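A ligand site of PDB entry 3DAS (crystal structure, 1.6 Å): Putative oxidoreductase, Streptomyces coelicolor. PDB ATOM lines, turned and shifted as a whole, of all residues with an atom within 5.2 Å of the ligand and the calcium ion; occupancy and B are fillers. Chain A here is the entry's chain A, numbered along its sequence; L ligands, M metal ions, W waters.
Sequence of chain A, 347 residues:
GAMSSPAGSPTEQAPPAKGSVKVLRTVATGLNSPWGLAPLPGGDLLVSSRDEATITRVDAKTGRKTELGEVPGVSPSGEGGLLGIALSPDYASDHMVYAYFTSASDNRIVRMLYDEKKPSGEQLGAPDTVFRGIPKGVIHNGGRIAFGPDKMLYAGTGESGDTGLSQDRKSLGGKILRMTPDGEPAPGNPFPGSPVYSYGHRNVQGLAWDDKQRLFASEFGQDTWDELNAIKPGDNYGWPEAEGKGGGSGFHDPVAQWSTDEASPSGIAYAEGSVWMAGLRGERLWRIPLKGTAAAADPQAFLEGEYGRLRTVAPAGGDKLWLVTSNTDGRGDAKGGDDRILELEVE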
ATOM      1  N   TRP A  35       7.501   7.015  -5.150  1.00  0.00           N
ATOM      2  CA  TRP A  35       7.549   8.386  -4.696  1.00  0.00           C
ATOM      3  C   TRP A  35       6.145   8.993  -4.686  1.00  0.00           C
ATOM      4  O   TRP A  35       5.537   9.132  -3.631  1.00  0.00           O
ATOM      5  CB  TRP A  35       8.519   9.179  -5.577  1.00  0.00           C
ATOM      6  CG  TRP A  35       9.242  10.297  -4.849  1.00  0.00           C
ATOM      7  CD1 TRP A  35      10.563  10.310  -4.469  1.00  0.00           C
ATOM      8  CD2 TRP A  35       8.701  11.564  -4.427  1.00  0.00           C
ATOM      9  NE1 TRP A  35      10.872  11.491  -3.840  1.00  0.00           N
ATOM     10  CE2 TRP A  35       9.750  12.287  -3.812  1.00  0.00           C
ATOM     11  CE3 TRP A  35       7.428  12.157  -4.522  1.00  0.00           C
ATOM     12  CZ2 TRP A  35       9.568  13.573  -3.283  1.00  0.00           C
ATOM     13  CZ3 TRP A  35       7.251  13.447  -4.002  1.00  0.00           C
ATOM     14  CH2 TRP A  35       8.318  14.132  -3.382  1.00  0.00           C
ATOM     15  N   ARG A  50      11.005   7.208  -8.743  1.00  0.00           N
ATOM     16  CA  ARG A  50      11.895   8.346  -8.900  1.00  0.00           C
ATOM     17  C   ARG A  50      13.020   8.054  -9.876  1.00  0.00           C
ATOM     18  O   ARG A  50      13.332   8.872 -10.742  1.00  0.00           O
ATOM     19  CB  ARG A  50      12.498   8.791  -7.563  1.00  0.00           C
ATOM     20  CG  ARG A  50      13.291  10.081  -7.666  1.00  0.00           C
ATOM     21  CD  ARG A  50      14.064  10.328  -6.375  1.00  0.00           C
ATOM     22  NE  ARG A  50      15.083   9.289  -6.192  1.00  0.00           N
ATOM     23  CZ  ARG A  50      15.670   9.012  -5.038  1.00  0.00           C
ATOM     24  NH1 ARG A  50      15.335   9.664  -3.926  1.00  0.00           N
ATOM     25  NH2 ARG A  50      16.575   8.037  -4.992  1.00  0.00           N
ATOM     26  N   GLU A  79      18.454  13.226  -4.879  1.00  0.00           N
ATOM     27  CA  GLU A  79      17.044  13.280  -4.462  1.00  0.00           C
ATOM     28  C   GLU A  79      16.110  13.648  -5.612  1.00  0.00           C
ATOM     29  O   GLU A  79      14.882  13.684  -5.449  1.00  0.00           O
ATOM     30  CB  GLU A  79      16.887  14.297  -3.320  1.00  0.00           C
ATOM     31  CG  GLU A  79      17.648  13.881  -2.069  1.00  0.00           C
ATOM     32  CD  GLU A  79      17.751  14.981  -1.022  1.00  0.00           C
ATOM     33  OE1 GLU A  79      17.076  16.033  -1.148  1.00  0.00           O
ATOM     34  OE2 GLU A  79      18.508  14.774  -0.050  1.00  0.00           O
ATOM     35  N   HIS A 140      17.395  18.615  -2.273  1.00  0.00           N
ATOM     36  CA  HIS A 140      16.399  19.666  -2.022  1.00  0.00           C
ATOM     37  C   HIS A 140      15.655  20.118  -3.258  1.00  0.00           C
ATOM     38  O   HIS A 140      15.648  21.308  -3.616  1.00  0.00           O
ATOM     39  CB  HIS A 140      17.000  20.861  -1.265  1.00  0.00           C
ATOM     40  CG  HIS A 140      17.600  20.493   0.053  1.00  0.00           C
ATOM     41  ND1 HIS A 140      18.287  21.394   0.830  1.00  0.00           N
ATOM     42  CD2 HIS A 140      17.646  19.310   0.726  1.00  0.00           C
ATOM     43  CE1 HIS A 140      18.715  20.809   1.930  1.00  0.00           C
ATOM     44  NE2 HIS A 140      18.352  19.540   1.893  1.00  0.00           N
ATOM     45  N   ARG A 202      12.707  25.130   3.436  1.00  0.00           N
ATOM     46  CA  ARG A 202      13.950  24.450   3.107  1.00  0.00           C
ATOM     47  C   ARG A 202      13.724  23.400   2.013  1.00  0.00           C
ATOM     48  O   ARG A 202      14.309  23.471   0.933  1.00  0.00           O
ATOM     49  CB  ARG A 202      14.543  23.817   4.368  1.00  0.00           C
ATOM     50  CG  ARG A 202      15.895  23.124   4.148  1.00  0.00           C
ATOM     51  CD  ARG A 202      16.475  22.723   5.489  1.00  0.00           C
ATOM     52  NE  ARG A 202      17.688  21.911   5.368  1.00  0.00           N
ATOM     53  CZ  ARG A 202      17.690  20.610   5.090  1.00  0.00           C
ATOM     54  NH1 ARG A 202      16.536  19.977   4.872  1.00  0.00           N
ATOM     55  NH2 ARG A 202      18.845  19.943   5.005  1.00  0.00           N
ATOM     56  N   ASN A 203      12.852  22.435   2.290  1.00  0.00           N
ATOM     57  CA  ASN A 203      12.581  21.350   1.353  1.00  0.00           C
ATOM     58  C   ASN A 203      11.258  20.736   1.762  1.00  0.00           C
ATOM     59  O   ASN A 203      11.130  20.201   2.872  1.00  0.00           O
ATOM     60  CB  ASN A 203      13.698  20.287   1.394  1.00  0.00           C
ATOM     61  CG  ASN A 203      13.640  19.335   0.194  1.00  0.00           C
ATOM     62  OD1 ASN A 203      13.162  19.704  -0.876  1.00  0.00           O
ATOM     63  ND2 ASN A 203      14.157  18.111   0.370  1.00  0.00           N
ATOM     64  N   GLN A 205       8.144  18.187   0.959  1.00  0.00           N
ATOM     65  CA  GLN A 205       7.692  16.985   0.249  1.00  0.00           C
ATOM     66  C   GLN A 205       6.368  16.430   0.761  1.00  0.00           C
ATOM     67  O   GLN A 205       6.047  15.266   0.523  1.00  0.00           O
ATOM     68  CB  GLN A 205       8.767  15.892   0.313  1.00  0.00           C
ATOM     69  CG  GLN A 205      10.059  16.199  -0.451  1.00  0.00           C
ATOM     70  CD  GLN A 205      11.030  15.024  -0.450  1.00  0.00           C
ATOM     71  OE1 GLN A 205      10.720  13.926   0.029  1.00  0.00           O
ATOM     72  NE2 GLN A 205      12.222  15.260  -0.981  1.00  0.00           N
ATOM     73  N   PHE A 220      11.601  19.087   5.752  1.00  0.00           N
ATOM     74  CA  PHE A 220      12.867  18.612   6.303  1.00  0.00           C
ATOM     75  C   PHE A 220      13.659  19.772   6.879  1.00  0.00           C
ATOM     76  O   PHE A 220      13.931  20.753   6.181  1.00  0.00           O
ATOM     77  CB  PHE A 220      13.748  17.975   5.230  1.00  0.00           C
ATOM     78  CG  PHE A 220      13.166  16.757   4.574  1.00  0.00           C
ATOM     79  CD1 PHE A 220      13.455  15.481   5.056  1.00  0.00           C
ATOM     80  CD2 PHE A 220      12.411  16.880   3.398  1.00  0.00           C
ATOM     81  CE1 PHE A 220      12.943  14.336   4.400  1.00  0.00           C
ATOM     82  CE2 PHE A 220      11.898  15.734   2.742  1.00  0.00           C
ATOM     83  CZ  PHE A 220      12.184  14.464   3.237  1.00  0.00           C
ATOM     84  N   GLY A 221      14.056  19.648   8.145  1.00  0.00           N
ATOM     85  CA  GLY A 221      15.047  20.541   8.733  1.00  0.00           C
ATOM     86  C   GLY A 221      16.454  20.085   8.383  1.00  0.00           C
ATOM     87  O   GLY A 221      16.644  19.077   7.680  1.00  0.00           O
ATOM     88  N   GLN A 222      17.438  20.807   8.909  1.00  0.00           N
ATOM     89  CA  GLN A 222      18.829  20.462   8.630  1.00  0.00           C
ATOM     90  C   GLN A 222      19.241  19.342   9.560  1.00  0.00           C
ATOM     91  O   GLN A 222      19.025  18.180   9.235  1.00  0.00           O
ATOM     92  CB  GLN A 222      19.729  21.695   8.738  1.00  0.00           C
ATOM     93  CG  GLN A 222      21.163  21.409   8.323  1.00  0.00           C
ATOM     94  CD  GLN A 222      21.956  22.673   8.120  1.00  0.00           C
ATOM     95  OE1 GLN A 222      21.751  23.407   7.148  1.00  0.00           O
ATOM     96  NE2 GLN A 222      22.876  22.950   9.034  1.00  0.00           N
ATOM     97  N   ASP A 223      19.785  19.676  10.734  1.00  0.00           N
ATOM     98  CA  ASP A 223      20.209  18.670  11.702  1.00  0.00           C
ATOM     99  C   ASP A 223      19.461  18.795  13.020  1.00  0.00           C
ATOM    100  O   ASP A 223      19.706  18.006  13.938  1.00  0.00           O
ATOM    101  CB  ASP A 223      21.713  18.799  11.981  1.00  0.00           C
ATOM    102  CG  ASP A 223      22.535  18.695  10.717  1.00  0.00           C
ATOM    103  OD1 ASP A 223      22.273  17.784   9.921  1.00  0.00           O
ATOM    104  OD2 ASP A 223      23.425  19.545  10.521  1.00  0.00           O
ATOM    105  N   ASP A 226      12.817  19.037  12.099  1.00  0.00           N
ATOM    106  CA  ASP A 226      11.830  18.900  11.025  1.00  0.00           C
ATOM    107  C   ASP A 226      10.536  19.545  11.471  1.00  0.00           C
ATOM    108  O   ASP A 226      10.310  19.741  12.664  1.00  0.00           O
ATOM    109  CB  ASP A 226      11.608  17.426  10.709  1.00  0.00           C
ATOM    110  CG  ASP A 226      12.871  16.743  10.277  1.00  0.00           C
ATOM    111  OD1 ASP A 226      13.601  17.310   9.435  1.00  0.00           O
ATOM    112  OD2 ASP A 226      13.131  15.626  10.768  1.00  0.00           O
ATOM    113  N   THR A 260      15.661  15.296  13.754  1.00  0.00           N
ATOM    114  CA  THR A 260      15.817  14.758  12.403  1.00  0.00           C
ATOM    115  C   THR A 260      15.947  13.231  12.369  1.00  0.00           C
ATOM    116  O   THR A 260      15.553  12.580  11.394  1.00  0.00           O
ATOM    117  CB  THR A 260      16.953  15.472  11.657  1.00  0.00           C
ATOM    118  OG1 THR A 260      18.161  15.341  12.404  1.00  0.00           O
ATOM    119  CG2 THR A 260      16.596  16.974  11.484  1.00  0.00           C
ATOM    120  N   SER A 264      12.511  13.205   9.683  1.00  0.00           N
ATOM    121  CA  SER A 264      12.921  13.492   8.303  1.00  0.00           C
ATOM    122  C   SER A 264      11.740  13.168   7.377  1.00  0.00           C
ATOM    123  O   SER A 264      11.755  12.165   6.635  1.00  0.00           O
ATOM    124  CB  SER A 264      14.222  12.771   7.913  1.00  0.00           C
ATOM    125  OG  SER A 264      15.323  13.242   8.688  1.00  0.00           O
ATOM    126  N   LEU A 280      11.228   9.283   6.839  1.00  0.00           N
ATOM    127  CA  LEU A 280      12.278   8.539   6.140  1.00  0.00           C
ATOM    128  C   LEU A 280      13.303   8.023   7.146  1.00  0.00           C
ATOM    129  O   LEU A 280      13.216   6.867   7.565  1.00  0.00           O
ATOM    130  CB  LEU A 280      12.941   9.376   5.025  1.00  0.00           C
ATOM    131  CG  LEU A 280      12.032   9.638   3.813  1.00  0.00           C
ATOM    132  CD1 LEU A 280      12.587  10.757   2.934  1.00  0.00           C
ATOM    133  CD2 LEU A 280      11.822   8.351   3.003  1.00  0.00           C
ATOM    134  N   ARG A 281      14.238   8.876   7.568  1.00  0.00           N
ATOM    135  CA  ARG A 281      15.207   8.475   8.584  1.00  0.00           C
ATOM    136  C   ARG A 281      14.515   7.982   9.849  1.00  0.00           C
ATOM    137  O   ARG A 281      14.990   7.031  10.497  1.00  0.00           O
ATOM    138  CB  ARG A 281      16.183   9.604   8.888  1.00  0.00           C
ATOM    139  CG  ARG A 281      17.290   9.168   9.817  1.00  0.00           C
ATOM    140  CD  ARG A 281      18.230  10.298  10.126  1.00  0.00           C
ATOM    141  NE  ARG A 281      19.035   9.987  11.302  1.00  0.00           N
ATOM    142  CZ  ARG A 281      19.934  10.813  11.842  1.00  0.00           C
ATOM    143  NH1 ARG A 281      20.142  11.994  11.292  1.00  0.00           N
ATOM    144  NH2 ARG A 281      20.621  10.456  12.914  1.00  0.00           N
ATOM    145  N   ARG A 309      12.273   2.819   6.042  1.00  0.00           N
ATOM    146  CA  ARG A 309      11.973   4.200   5.642  1.00  0.00           C
ATOM    147  C   ARG A 309      10.570   4.321   5.052  1.00  0.00           C
ATOM    148  O   ARG A 309      10.143   3.458   4.282  1.00  0.00           O
ATOM    149  CB  ARG A 309      13.000   4.668   4.611  1.00  0.00           C
ATOM    150  CG  ARG A 309      14.429   4.705   5.155  1.00  0.00           C
ATOM    151  CD  ARG A 309      15.459   4.782   4.025  1.00  0.00           C
ATOM    152  NE  ARG A 309      15.352   5.981   3.186  1.00  0.00           N
ATOM    153  CZ  ARG A 309      15.697   7.217   3.561  1.00  0.00           C
ATOM    154  NH1 ARG A 309      16.148   7.448   4.793  1.00  0.00           N
ATOM    155  NH2 ARG A 309      15.577   8.220   2.707  1.00  0.00           N
ATOM    156  N   ARG A 311       7.985   6.960   2.939  1.00  0.00           N
ATOM    157  CA  ARG A 311       8.020   8.184   2.133  1.00  0.00           C
ATOM    158  C   ARG A 311       6.673   8.835   1.884  1.00  0.00           C
ATOM    159  O   ARG A 311       6.559  10.062   1.858  1.00  0.00           O
ATOM    160  CB  ARG A 311       8.741   7.966   0.804  1.00  0.00           C
ATOM    161  CG  ARG A 311       8.810   9.266  -0.021  1.00  0.00           C
ATOM    162  CD  ARG A 311       9.633   9.117  -1.244  1.00  0.00           C
ATOM    163  NE  ARG A 311      11.036   8.868  -0.968  1.00  0.00           N
ATOM    164  CZ  ARG A 311      11.961   9.811  -0.772  1.00  0.00           C
ATOM    165  NH1 ARG A 311      11.630  11.118  -0.759  1.00  0.00           N
ATOM    166  NH2 ARG A 311      13.225   9.440  -0.560  1.00  0.00           N
ATOM    167  N   ASP A 329      15.490   3.814  -2.096  1.00  0.00           N
ATOM    168  CA  ASP A 329      15.755   5.175  -2.587  1.00  0.00           C
ATOM    169  C   ASP A 329      17.237   5.595  -2.481  1.00  0.00           C
ATOM    170  O   ASP A 329      17.560   6.771  -2.664  1.00  0.00           O
ATOM    171  CB  ASP A 329      14.862   6.203  -1.872  1.00  0.00           C
ATOM    172  CG  ASP A 329      15.181   6.358  -0.390  1.00  0.00           C
ATOM    173  OD1 ASP A 329      16.197   5.814   0.082  1.00  0.00           O
ATOM    174  OD2 ASP A 329      14.395   7.030   0.329  1.00  0.00           O
ATOM    175  N   ARG A 331      19.095   5.283   0.283  1.00  0.00           N
ATOM    176  CA  ARG A 331      19.456   5.525   1.681  1.00  0.00           C
ATOM    177  C   ARG A 331      18.896   4.472   2.626  1.00  0.00           C
ATOM    178  O   ARG A 331      18.938   4.651   3.843  1.00  0.00           O
ATOM    179  CB  ARG A 331      19.003   6.919   2.103  1.00  0.00           C
ATOM    180  CG  ARG A 331      19.748   8.018   1.351  1.00  0.00           C
ATOM    181  CD  ARG A 331      19.261   9.393   1.731  1.00  0.00           C
ATOM    182  NE  ARG A 331      19.959  10.398   0.932  1.00  0.00           N
ATOM    183  CZ  ARG A 331      19.570  11.676   0.820  1.00  0.00           C
ATOM    184  NH1 ARG A 331      18.494  12.099   1.462  1.00  0.00           N
ATOM    185  NH2 ARG A 331      20.253  12.505   0.052  1.00  0.00           N
HETATM  186  N1  LIG L   1      15.666  12.809   2.306  1.00  0.00           N
HETATM  187  C1  LIG L   1      15.150  13.371   1.182  1.00  0.00           C
HETATM  188  C2  LIG L   1      14.652  12.551   0.052  1.00  0.00           C
HETATM  189  O1  LIG L   1      15.034  11.362   0.064  1.00  0.00           O
HETATM  190  O2  LIG L   1      14.018  13.061  -0.891  1.00  0.00           O
HETATM  191  C3  LIG L   1      15.210  14.771   1.204  1.00  0.00           C
HETATM  192  C4  LIG L   1      15.827  15.044   2.454  1.00  0.00           C
HETATM  193  C5  LIG L   1      16.103  13.768   3.128  1.00  0.00           C
HETATM  194  C6  LIG L   1      16.186  16.324   3.122  1.00  0.00           C
HETATM  195  O3  LIG L   1      15.929  17.432   2.565  1.00  0.00           O
HETATM  196  C7  LIG L   1      16.823  16.253   4.455  1.00  0.00           C
HETATM  197  O4  LIG L   1      17.160  17.290   5.092  1.00  0.00           O
HETATM  198  C8  LIG L   1      17.074  14.915   5.059  1.00  0.00           C
HETATM  199  N2  LIG L   1      17.652  14.876   6.261  1.00  0.00           N
HETATM  200  C9  LIG L   1      17.921  13.727   6.892  1.00  0.00           C
HETATM  201  C10 LIG L   1      18.584  13.897   8.219  1.00  0.00           C
HETATM  202  O5  LIG L   1      18.718  15.080   8.645  1.00  0.00           O
HETATM  203  O6  LIG L   1      19.049  12.902   8.802  1.00  0.00           O
HETATM  204  C11 LIG L   1      17.617  12.481   6.361  1.00  0.00           C
HETATM  205  C12 LIG L   1      17.015  12.381   5.104  1.00  0.00           C
HETATM  206  C13 LIG L   1      16.713  10.995   4.619  1.00  0.00           C
HETATM  207  O7  LIG L   1      16.362  10.184   5.503  1.00  0.00           O
HETATM  208  O8  LIG L   1      16.792  10.710   3.408  1.00  0.00           O
HETATM  209  C14 LIG L   1      16.702  13.653   4.381  1.00  0.00           C
HETATM  210 CA    CA M   1      17.809  17.018   7.441  1.00  0.00          CA
HETATM  211  O   HOH W   1      16.700   9.531  -1.253  1.00  0.00           O
HETATM  212  O   HOH W   2      20.873  11.239   7.672  1.00  0.00           O
HETATM  213  O   HOH W   3      19.986  17.298   6.393  1.00  0.00           O
HETATM  214  O   HOH W   4      19.002   8.971   6.227  1.00  0.00           O
HETATM  215  O   HOH W   5      15.693  16.079   8.282  1.00  0.00           O
HETATM  216  O   HOH W   6      13.723  12.084  -3.449  1.00  0.00           O
HETATM  217  O   HOH W   7      19.843  17.742   3.444  1.00  0.00           O
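The guanidinium group (NH2) of Arg 311 is in salt-bridge range of an oxygen (O1) of the ligand (2.7 Å). The guanidinium group (NH1) of Arg 202 lies within hydrogen-bond range of an oxygen (O3) of the ligand (3.5 Å). The guanidinium group (NH1) of Arg 309 is in salt-bridge range of an oxygen (O7) of the ligand. An oxygen (O2) of the ligand sits at hydrogen-bond distance from the side-chain amide nitrogen of Gln 205, 2.8 Å away. The backbone NH of Arg 281 lies within hydrogen-bond range of an oxygen (O7) of the ligand (3.2 Å). O6 of the ligand lies within salt-bridge range of NH1 of Arg 281 (2.9 Å). The side-chain amide nitrogen (ND2) of Asn 203 is in hydrogen-bond range of an oxygen (O3) of the ligand, 2.9 Å away. NH1 of Arg 331 is in salt-bridge range of O8 of the ligand, 2.9 Å away. NE2 of His 140 lies close to O3 of the ligand (3.3 Å).
The backbone carbonyl oxygen (O) of Gly 221 lies close to the guanidinium group (NH1) of Arg 202 (3.0 Å). NH1 of Arg 311 lies within hydrogen-bond range of OE1 of Gln 205 (3.1 Å). NH2 of Arg 202 is in hydrogen-bond range of NE2 of His 140, at 3.2 Å. The backbone carbonyl oxygen of Phe 220 sits at hydrogen-bond distance from the guanidinium group of Arg 202, 3.0 Å away. The backbone NH of Arg 331 is in hydrogen-bond range of the side-chain carboxylate of Asp 329. OE1 of Glu 79 is in hydrogen-bond range of N of His 140 (2.8 Å). The backbone carbonyl oxygen (O) of Ser 264 is in hydrogen-bond range of the backbone NH (N) of Leu 280 (2.9 Å). OG1 of Thr 260 sits at hydrogen-bond distance from O of Asp 223, at 3.4 Å.
Merely in contact with the ligand: Ser 264, Glu 79, Phe 220, Thr 260 and Leu 280. Hydrophobic or aromatic side chains that line the ligand: His 140, Phe 220 and Leu 280. Of the 20 residues printed, 15 come within 4 Å of the ligand.
Arg 202 touches the calcium ion. Of the 20 residues printed, 3 come within 4 Å of the calcium ion.
The calcium ion is bound by O of Gly 221, 2.4 Å away. Water W3 binds the calcium ion, 2.4 Å away. The calcium ion is bound by N2 of the ligand (2.5 Å). The calcium ion is bound by an oxygen (O4) of the ligand, at 2.5 Å. The calcium ion is bound by an oxygen (O5) of the ligand, 2.5 Å away. O of Gln 222 is bound to the calcium ion (2.5 Å). Water W5 is bound to the calcium ion, at 2.5 Å. The calcium ion has seven donor atoms within binding distance.
Water W5 bridges OD1 of Asp 226 and OG of Ser 264. Water W6 lies within hydrogen-bond range of an oxygen (O2) of the ligand (2.8 Å), the backbone carbonyl oxygen of Glu 79 (2.8 Å), the indole nitrogen of Trp 35 (2.9 Å) and the guanidinium group of Arg 50 (2.9 Å). Water W1 lies within hydrogen-bond range of O1 of the ligand (2.8 Å), NH1 of Arg 50 (3.0 Å) and O of Asp 329 (3.2 Å). Water W7 bridges NE2 of His 140 (2.8 Å) and NH2 of Arg 202 (2.9 Å).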
